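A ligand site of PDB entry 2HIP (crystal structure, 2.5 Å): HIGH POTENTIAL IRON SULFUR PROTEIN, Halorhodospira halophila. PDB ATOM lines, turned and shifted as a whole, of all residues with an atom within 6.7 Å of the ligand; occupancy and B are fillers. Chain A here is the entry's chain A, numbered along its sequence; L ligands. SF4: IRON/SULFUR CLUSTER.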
ATOM      1  N   ALA A   9     -12.633 -24.353  15.178  1.00  0.00           N
ATOM      2  CA  ALA A   9     -13.360 -24.735  16.376  1.00  0.00           C
ATOM      3  C   ALA A   9     -14.848 -24.616  16.153  1.00  0.00           C
ATOM      4  O   ALA A   9     -15.292 -23.813  15.348  1.00  0.00           O
ATOM      5  CB  ALA A   9     -12.927 -23.885  17.555  1.00  0.00           C
ATOM      6  N   HIS A  10     -15.628 -25.413  16.841  1.00  0.00           N
ATOM      7  CA  HIS A  10     -17.067 -25.319  16.667  1.00  0.00           C
ATOM      8  C   HIS A  10     -17.585 -25.258  15.260  1.00  0.00           C
ATOM      9  O   HIS A  10     -18.446 -24.410  14.990  1.00  0.00           O
ATOM     10  CB  HIS A  10     -17.671 -24.119  17.400  1.00  0.00           C
ATOM     11  CG  HIS A  10     -17.149 -23.989  18.762  1.00  0.00           C
ATOM     12  ND1 HIS A  10     -17.607 -24.796  19.784  1.00  0.00           N
ATOM     13  CD2 HIS A  10     -16.203 -23.157  19.250  1.00  0.00           C
ATOM     14  CE1 HIS A  10     -16.933 -24.438  20.863  1.00  0.00           C
ATOM     15  NE2 HIS A  10     -16.083 -23.459  20.588  1.00  0.00           N
ATOM     16  N   TYR A  12     -16.301 -24.116  12.407  1.00  0.00           N
ATOM     17  CA  TYR A  12     -15.967 -22.874  11.701  1.00  0.00           C
ATOM     18  C   TYR A  12     -15.746 -22.949  10.183  1.00  0.00           C
ATOM     19  O   TYR A  12     -15.057 -23.831   9.669  1.00  0.00           O
ATOM     20  CB  TYR A  12     -14.724 -22.241  12.294  1.00  0.00           C
ATOM     21  CG  TYR A  12     -14.446 -20.917  11.668  1.00  0.00           C
ATOM     22  CD1 TYR A  12     -15.151 -19.794  12.103  1.00  0.00           C
ATOM     23  CD2 TYR A  12     -13.509 -20.782  10.645  1.00  0.00           C
ATOM     24  CE1 TYR A  12     -14.947 -18.525  11.553  1.00  0.00           C
ATOM     25  CE2 TYR A  12     -13.283 -19.528  10.080  1.00  0.00           C
ATOM     26  CZ  TYR A  12     -14.003 -18.411  10.539  1.00  0.00           C
ATOM     27  OH  TYR A  12     -13.769 -17.186   9.980  1.00  0.00           O
ATOM     28  N   LEU A  30     -24.074 -14.314  10.671  1.00  0.00           N
ATOM     29  CA  LEU A  30     -22.678 -14.032  10.389  1.00  0.00           C
ATOM     30  C   LEU A  30     -21.887 -13.533  11.579  1.00  0.00           C
ATOM     31  O   LEU A  30     -22.429 -12.938  12.508  1.00  0.00           O
ATOM     32  CB  LEU A  30     -22.667 -12.848   9.408  1.00  0.00           C
ATOM     33  CG  LEU A  30     -22.234 -13.163   7.993  1.00  0.00           C
ATOM     34  CD1 LEU A  30     -22.324 -14.654   7.733  1.00  0.00           C
ATOM     35  CD2 LEU A  30     -23.127 -12.407   7.016  1.00  0.00           C
ATOM     36  N   CYS A  31     -20.588 -13.741  11.525  1.00  0.00           N
ATOM     37  CA  CYS A  31     -19.718 -13.294  12.591  1.00  0.00           C
ATOM     38  C   CYS A  31     -19.892 -11.829  12.913  1.00  0.00           C
ATOM     39  O   CYS A  31     -19.814 -11.431  14.065  1.00  0.00           O
ATOM     40  CB  CYS A  31     -18.242 -13.522  12.226  1.00  0.00           C
ATOM     41  SG  CYS A  31     -17.731 -15.241  12.347  1.00  0.00           S
ATOM     42  N   GLU A  32     -20.071 -11.025  11.880  1.00  0.00           N
ATOM     43  CA  GLU A  32     -20.212  -9.592  12.079  1.00  0.00           C
ATOM     44  C   GLU A  32     -21.505  -9.136  12.761  1.00  0.00           C
ATOM     45  O   GLU A  32     -21.647  -7.995  13.185  1.00  0.00           O
ATOM     46  CB  GLU A  32     -19.829  -8.770  10.839  1.00  0.00           C
ATOM     47  CG  GLU A  32     -21.059  -8.395   9.999  1.00  0.00           C
ATOM     48  CD  GLU A  32     -20.727  -7.903   8.633  1.00  0.00           C
ATOM     49  OE1 GLU A  32     -19.501  -7.452   8.533  1.00  0.00           O
ATOM     50  OE2 GLU A  32     -21.520  -7.894   7.723  1.00  0.00           O
ATOM     51  N   CYS A  34     -22.694 -11.231  15.148  1.00  0.00           N
ATOM     52  CA  CYS A  34     -22.649 -12.137  16.271  1.00  0.00           C
ATOM     53  C   CYS A  34     -22.240 -11.414  17.522  1.00  0.00           C
ATOM     54  O   CYS A  34     -21.467 -10.456  17.491  1.00  0.00           O
ATOM     55  CB  CYS A  34     -21.710 -13.324  15.993  1.00  0.00           C
ATOM     56  SG  CYS A  34     -21.369 -14.340  17.452  1.00  0.00           S
ATOM     57  N   ALA A  35     -22.746 -11.879  18.622  1.00  0.00           N
ATOM     58  CA  ALA A  35     -22.438 -11.270  19.861  1.00  0.00           C
ATOM     59  C   ALA A  35     -20.964 -11.412  20.273  1.00  0.00           C
ATOM     60  O   ALA A  35     -20.467 -10.576  21.023  1.00  0.00           O
ATOM     61  CB  ALA A  35     -23.376 -11.753  20.951  1.00  0.00           C
ATOM     62  N   PHE A  36     -20.258 -12.448  19.800  1.00  0.00           N
ATOM     63  CA  PHE A  36     -18.850 -12.611  20.175  1.00  0.00           C
ATOM     64  C   PHE A  36     -17.895 -11.740  19.365  1.00  0.00           C
ATOM     65  O   PHE A  36     -16.704 -11.658  19.669  1.00  0.00           O
ATOM     66  CB  PHE A  36     -18.377 -14.067  20.151  1.00  0.00           C
ATOM     67  CG  PHE A  36     -18.833 -14.909  21.326  1.00  0.00           C
ATOM     68  CD1 PHE A  36     -18.244 -14.763  22.580  1.00  0.00           C
ATOM     69  CD2 PHE A  36     -19.828 -15.869  21.173  1.00  0.00           C
ATOM     70  CE1 PHE A  36     -18.629 -15.550  23.668  1.00  0.00           C
ATOM     71  CE2 PHE A  36     -20.236 -16.659  22.246  1.00  0.00           C
ATOM     72  CZ  PHE A  36     -19.640 -16.501  23.499  1.00  0.00           C
ATOM     73  N   TRP A  37     -18.413 -11.107  18.323  1.00  0.00           N
ATOM     74  CA  TRP A  37     -17.646 -10.240  17.425  1.00  0.00           C
ATOM     75  C   TRP A  37     -17.073  -8.996  18.083  1.00  0.00           C
ATOM     76  O   TRP A  37     -17.787  -8.191  18.681  1.00  0.00           O
ATOM     77  CB  TRP A  37     -18.538  -9.858  16.267  1.00  0.00           C
ATOM     78  CG  TRP A  37     -18.006  -8.920  15.253  1.00  0.00           C
ATOM     79  CD1 TRP A  37     -18.403  -7.635  15.096  1.00  0.00           C
ATOM     80  CD2 TRP A  37     -17.086  -9.200  14.206  1.00  0.00           C
ATOM     81  NE1 TRP A  37     -17.762  -7.081  14.040  1.00  0.00           N
ATOM     82  CE2 TRP A  37     -16.952  -8.022  13.474  1.00  0.00           C
ATOM     83  CE3 TRP A  37     -16.361 -10.335  13.838  1.00  0.00           C
ATOM     84  CZ2 TRP A  37     -16.099  -7.952  12.387  1.00  0.00           C
ATOM     85  CZ3 TRP A  37     -15.517 -10.267  12.753  1.00  0.00           C
ATOM     86  CH2 TRP A  37     -15.391  -9.083  12.043  1.00  0.00           C
ATOM     87  N   GLY A  38     -15.744  -8.849  17.955  1.00  0.00           N
ATOM     88  CA  GLY A  38     -15.015  -7.724  18.518  1.00  0.00           C
ATOM     89  C   GLY A  38     -14.546  -6.695  17.473  1.00  0.00           C
ATOM     90  O   GLY A  38     -13.560  -5.980  17.678  1.00  0.00           O
ATOM     91  N   ARG A  47     -11.865  -9.761  15.592  1.00  0.00           N
ATOM     92  CA  ARG A  47     -11.649 -10.591  16.759  1.00  0.00           C
ATOM     93  C   ARG A  47     -12.904 -11.316  17.163  1.00  0.00           C
ATOM     94  O   ARG A  47     -14.022 -10.915  16.842  1.00  0.00           O
ATOM     95  CB  ARG A  47     -11.087  -9.816  17.955  1.00  0.00           C
ATOM     96  CG  ARG A  47     -10.037  -8.806  17.530  1.00  0.00           C
ATOM     97  CD  ARG A  47      -9.224  -8.258  18.687  1.00  0.00           C
ATOM     98  NE  ARG A  47      -8.021  -7.553  18.263  1.00  0.00           N
ATOM     99  CZ  ARG A  47      -7.603  -6.431  18.850  1.00  0.00           C
ATOM    100  NH1 ARG A  47      -8.264  -5.881  19.857  1.00  0.00           N
ATOM    101  NH2 ARG A  47      -6.491  -5.849  18.402  1.00  0.00           N
ATOM    102  N   CYS A  48     -12.702 -12.404  17.891  1.00  0.00           N
ATOM    103  CA  CYS A  48     -13.760 -13.241  18.428  1.00  0.00           C
ATOM    104  C   CYS A  48     -13.513 -13.253  19.953  1.00  0.00           C
ATOM    105  O   CYS A  48     -12.438 -13.675  20.386  1.00  0.00           O
ATOM    106  CB  CYS A  48     -13.755 -14.665  17.829  1.00  0.00           C
ATOM    107  SG  CYS A  48     -15.267 -15.594  18.224  1.00  0.00           S
ATOM    108  N   THR A  49     -14.476 -12.788  20.792  1.00  0.00           N
ATOM    109  CA  THR A  49     -14.292 -12.759  22.273  1.00  0.00           C
ATOM    110  C   THR A  49     -14.425 -14.129  22.976  1.00  0.00           C
ATOM    111  O   THR A  49     -14.152 -14.247  24.171  1.00  0.00           O
ATOM    112  CB  THR A  49     -15.090 -11.667  23.007  1.00  0.00           C
ATOM    113  OG1 THR A  49     -16.322 -12.195  23.455  1.00  0.00           O
ATOM    114  CG2 THR A  49     -15.319 -10.464  22.106  1.00  0.00           C
ATOM    115  N   HIS A  50     -14.846 -15.138  22.178  1.00  0.00           N
ATOM    116  CA  HIS A  50     -15.026 -16.523  22.614  1.00  0.00           C
ATOM    117  C   HIS A  50     -13.634 -17.112  22.768  1.00  0.00           C
ATOM    118  O   HIS A  50     -12.812 -17.046  21.863  1.00  0.00           O
ATOM    119  CB  HIS A  50     -15.865 -17.321  21.617  1.00  0.00           C
ATOM    120  CG  HIS A  50     -16.145 -18.650  22.183  1.00  0.00           C
ATOM    121  ND1 HIS A  50     -15.137 -19.568  22.373  1.00  0.00           N
ATOM    122  CD2 HIS A  50     -17.316 -19.192  22.605  1.00  0.00           C
ATOM    123  CE1 HIS A  50     -15.700 -20.641  22.915  1.00  0.00           C
ATOM    124  NE2 HIS A  50     -17.011 -20.444  23.043  1.00  0.00           N
ATOM    125  N   PHE A  53     -11.555 -19.114  20.193  1.00  0.00           N
ATOM    126  CA  PHE A  53     -11.105 -18.375  19.015  1.00  0.00           C
ATOM    127  C   PHE A  53     -10.161 -17.242  19.373  1.00  0.00           C
ATOM    128  O   PHE A  53     -10.112 -16.224  18.695  1.00  0.00           O
ATOM    129  CB  PHE A  53     -12.439 -17.717  18.500  1.00  0.00           C
ATOM    130  CG  PHE A  53     -13.320 -18.740  17.803  1.00  0.00           C
ATOM    131  CD1 PHE A  53     -12.893 -19.143  16.540  1.00  0.00           C
ATOM    132  CD2 PHE A  53     -14.484 -19.301  18.326  1.00  0.00           C
ATOM    133  CE1 PHE A  53     -13.583 -20.096  15.789  1.00  0.00           C
ATOM    134  CE2 PHE A  53     -15.190 -20.258  17.590  1.00  0.00           C
ATOM    135  CZ  PHE A  53     -14.735 -20.645  16.331  1.00  0.00           C
ATOM    136  N   VAL A  58     -10.956 -13.931  12.781  1.00  0.00           N
ATOM    137  CA  VAL A  58     -12.131 -14.561  12.213  1.00  0.00           C
ATOM    138  C   VAL A  58     -12.575 -13.671  11.041  1.00  0.00           C
ATOM    139  O   VAL A  58     -12.179 -12.509  10.976  1.00  0.00           O
ATOM    140  CB  VAL A  58     -13.231 -14.838  13.237  1.00  0.00           C
ATOM    141  CG1 VAL A  58     -12.697 -15.685  14.390  1.00  0.00           C
ATOM    142  CG2 VAL A  58     -13.806 -13.528  13.762  1.00  0.00           C
ATOM    143  N   LYS A  59     -13.394 -14.192  10.114  1.00  0.00           N
ATOM    144  CA  LYS A  59     -13.849 -13.418   8.949  1.00  0.00           C
ATOM    145  C   LYS A  59     -15.289 -12.922   8.988  1.00  0.00           C
ATOM    146  O   LYS A  59     -16.219 -13.690   9.240  1.00  0.00           O
ATOM    147  CB  LYS A  59     -13.686 -14.303   7.749  1.00  0.00           C
ATOM    148  CG  LYS A  59     -14.211 -13.670   6.493  1.00  0.00           C
ATOM    149  CD  LYS A  59     -13.067 -13.273   5.607  1.00  0.00           C
ATOM    150  CE  LYS A  59     -13.348 -13.565   4.149  1.00  0.00           C
ATOM    151  NZ  LYS A  59     -14.394 -12.692   3.605  1.00  0.00           N
ATOM    152  N   GLY A  62     -17.865 -15.175   7.965  1.00  0.00           N
ATOM    153  CA  GLY A  62     -17.729 -16.520   8.533  1.00  0.00           C
ATOM    154  C   GLY A  62     -18.920 -16.929   9.429  1.00  0.00           C
ATOM    155  O   GLY A  62     -19.915 -16.217   9.484  1.00  0.00           O
ATOM    156  N   TRP A  63     -18.822 -18.108  10.106  1.00  0.00           N
ATOM    157  CA  TRP A  63     -19.869 -18.669  11.002  1.00  0.00           C
ATOM    158  C   TRP A  63     -19.321 -19.848  11.797  1.00  0.00           C
ATOM    159  O   TRP A  63     -18.605 -20.681  11.269  1.00  0.00           O
ATOM    160  CB  TRP A  63     -21.106 -19.168  10.218  1.00  0.00           C
ATOM    161  CG  TRP A  63     -22.332 -19.556  11.031  1.00  0.00           C
ATOM    162  CD1 TRP A  63     -23.364 -18.736  11.367  1.00  0.00           C
ATOM    163  CD2 TRP A  63     -22.681 -20.847  11.573  1.00  0.00           C
ATOM    164  NE1 TRP A  63     -24.321 -19.401  12.073  1.00  0.00           N
ATOM    165  CE2 TRP A  63     -23.929 -20.708  12.230  1.00  0.00           C
ATOM    166  CE3 TRP A  63     -22.059 -22.093  11.554  1.00  0.00           C
ATOM    167  CZ2 TRP A  63     -24.538 -21.792  12.885  1.00  0.00           C
ATOM    168  CZ3 TRP A  63     -22.651 -23.153  12.217  1.00  0.00           C
ATOM    169  CH2 TRP A  63     -23.900 -23.010  12.832  1.00  0.00           C
ATOM    170  N   CYS A  64     -19.691 -19.888  13.089  1.00  0.00           N
ATOM    171  CA  CYS A  64     -19.291 -20.941  14.027  1.00  0.00           C
ATOM    172  C   CYS A  64     -20.534 -21.395  14.739  1.00  0.00           C
ATOM    173  O   CYS A  64     -21.417 -20.587  15.018  1.00  0.00           O
ATOM    174  CB  CYS A  64     -18.185 -20.557  15.034  1.00  0.00           C
ATOM    175  SG  CYS A  64     -18.804 -19.768  16.535  1.00  0.00           S
ATOM    176  N   SER A  65     -20.585 -22.678  15.066  1.00  0.00           N
ATOM    177  CA  SER A  65     -21.741 -23.280  15.719  1.00  0.00           C
ATOM    178  C   SER A  65     -22.139 -22.639  17.047  1.00  0.00           C
ATOM    179  O   SER A  65     -23.241 -22.875  17.559  1.00  0.00           O
ATOM    180  CB  SER A  65     -21.617 -24.788  15.818  1.00  0.00           C
ATOM    181  OG  SER A  65     -20.755 -25.147  16.872  1.00  0.00           O
ATOM    182  N   VAL A  66     -21.241 -21.837  17.618  1.00  0.00           N
ATOM    183  CA  VAL A  66     -21.533 -21.184  18.870  1.00  0.00           C
ATOM    184  C   VAL A  66     -21.936 -19.761  18.658  1.00  0.00           C
ATOM    185  O   VAL A  66     -21.626 -18.882  19.466  1.00  0.00           O
ATOM    186  CB  VAL A  66     -20.447 -21.286  19.942  1.00  0.00           C
ATOM    187  CG1 VAL A  66     -20.130 -22.739  20.255  1.00  0.00           C
ATOM    188  CG2 VAL A  66     -19.192 -20.529  19.529  1.00  0.00           C
ATOM    189  N   TYR A  67     -22.599 -19.536  17.541  1.00  0.00           N
ATOM    190  CA  TYR A  67     -23.089 -18.222  17.191  1.00  0.00           C
ATOM    191  C   TYR A  67     -24.178 -17.801  18.172  1.00  0.00           C
ATOM    192  O   TYR A  67     -24.953 -18.629  18.662  1.00  0.00           O
ATOM    193  CB  TYR A  67     -23.688 -18.249  15.749  1.00  0.00           C
ATOM    194  CG  TYR A  67     -24.374 -16.952  15.312  1.00  0.00           C
ATOM    195  CD1 TYR A  67     -23.606 -15.874  14.886  1.00  0.00           C
ATOM    196  CD2 TYR A  67     -25.773 -16.823  15.304  1.00  0.00           C
ATOM    197  CE1 TYR A  67     -24.225 -14.688  14.480  1.00  0.00           C
ATOM    198  CE2 TYR A  67     -26.409 -15.643  14.912  1.00  0.00           C
ATOM    199  CZ  TYR A  67     -25.615 -14.580  14.489  1.00  0.00           C
ATOM    200  OH  TYR A  67     -26.206 -13.409  14.096  1.00  0.00           O
ATOM    201  N   ALA A  68     -24.217 -16.505  18.434  1.00  0.00           N
ATOM    202  CA  ALA A  68     -25.180 -15.869  19.321  1.00  0.00           C
ATOM    203  C   ALA A  68     -25.576 -14.530  18.724  1.00  0.00           C
ATOM    204  O   ALA A  68     -24.714 -13.743  18.335  1.00  0.00           O
ATOM    205  CB  ALA A  68     -24.622 -15.715  20.728  1.00  0.00           C
HETATM  206 FE1  SF4 L   1     -17.928 -15.765  14.451  1.00  0.00          FE
HETATM  207 FE2  SF4 L   1     -19.435 -15.507  16.606  1.00  0.00          FE
HETATM  208 FE3  SF4 L   1     -16.823 -15.893  16.866  1.00  0.00          FE
HETATM  209 FE4  SF4 L   1     -18.379 -17.871  15.991  1.00  0.00          FE
HETATM  210  S1  SF4 L   1     -18.438 -16.919  17.992  1.00  0.00           S
HETATM  211  S2  SF4 L   1     -16.429 -17.239  15.148  1.00  0.00           S
HETATM  212  S3  SF4 L   1     -19.888 -16.744  14.818  1.00  0.00           S
HETATM  213  S4  SF4 L   1     -17.822 -14.136  15.948  1.00  0.00           S
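N of Cys 64 lies close to S3 of the ligand, at 3.6 Å. The side-chain sulfur of Cys 64 binds an iron atom (FE4) of the ligand, at 2.0 Å. An iron atom (FE3) of the ligand is bound by the side-chain sulfur (SG) of Cys 48, 2.1 Å away. The side-chain sulfur (SG) of Cys 31 is bound to an iron atom (FE1) of the ligand, at 2.2 Å. SG of Cys 34 binds FE2 of the ligand (2.4 Å).
The side-chain sulfur of Cys 64 sits close to the backbone NH of Val 66 (3.4 Å). The side-chain sulfur (SG) of Cys 31 sits close to the backbone NH (N) of Trp 63, at 3.8 Å. The backbone NH (N) of Cys 31 is in hydrogen-bond range of the backbone carbonyl oxygen (O) of Gly 62 (3.3 Å). The side-chain sulfur (SG) of Cys 31 lies close to the backbone carbonyl oxygen (O) of Lys 59, 3.8 Å away. N of Phe 36 lies close to SG of Cys 34 (3.2 Å). The backbone carbonyl oxygen (O) of Ala 68 sits close to the side-chain sulfur (SG) of Cys 34 (3.5 Å). The backbone carbonyl oxygen of Phe 36 lies within hydrogen-bond range of the backbone NH of Thr 49.
CB of Phe 36 touches S1 of the ligand (3.6 Å). N of Trp 37 touches S4 of the ligand, at 3.9 Å. CZ of Phe 53 touches S2 of the ligand, at 3.98 Å. CG2 of Val 66 touches S1 of the ligand, 3.995 Å away. CD1 of Tyr 67 touches S3 of the ligand (3.8 Å). Hydrophobic or aromatic side chains that line the ligand: Phe 36, Phe 53, Val 66 and Tyr 67. The nearest printed residue that does not touch the ligand is Tyr 12 (4.1 Å).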
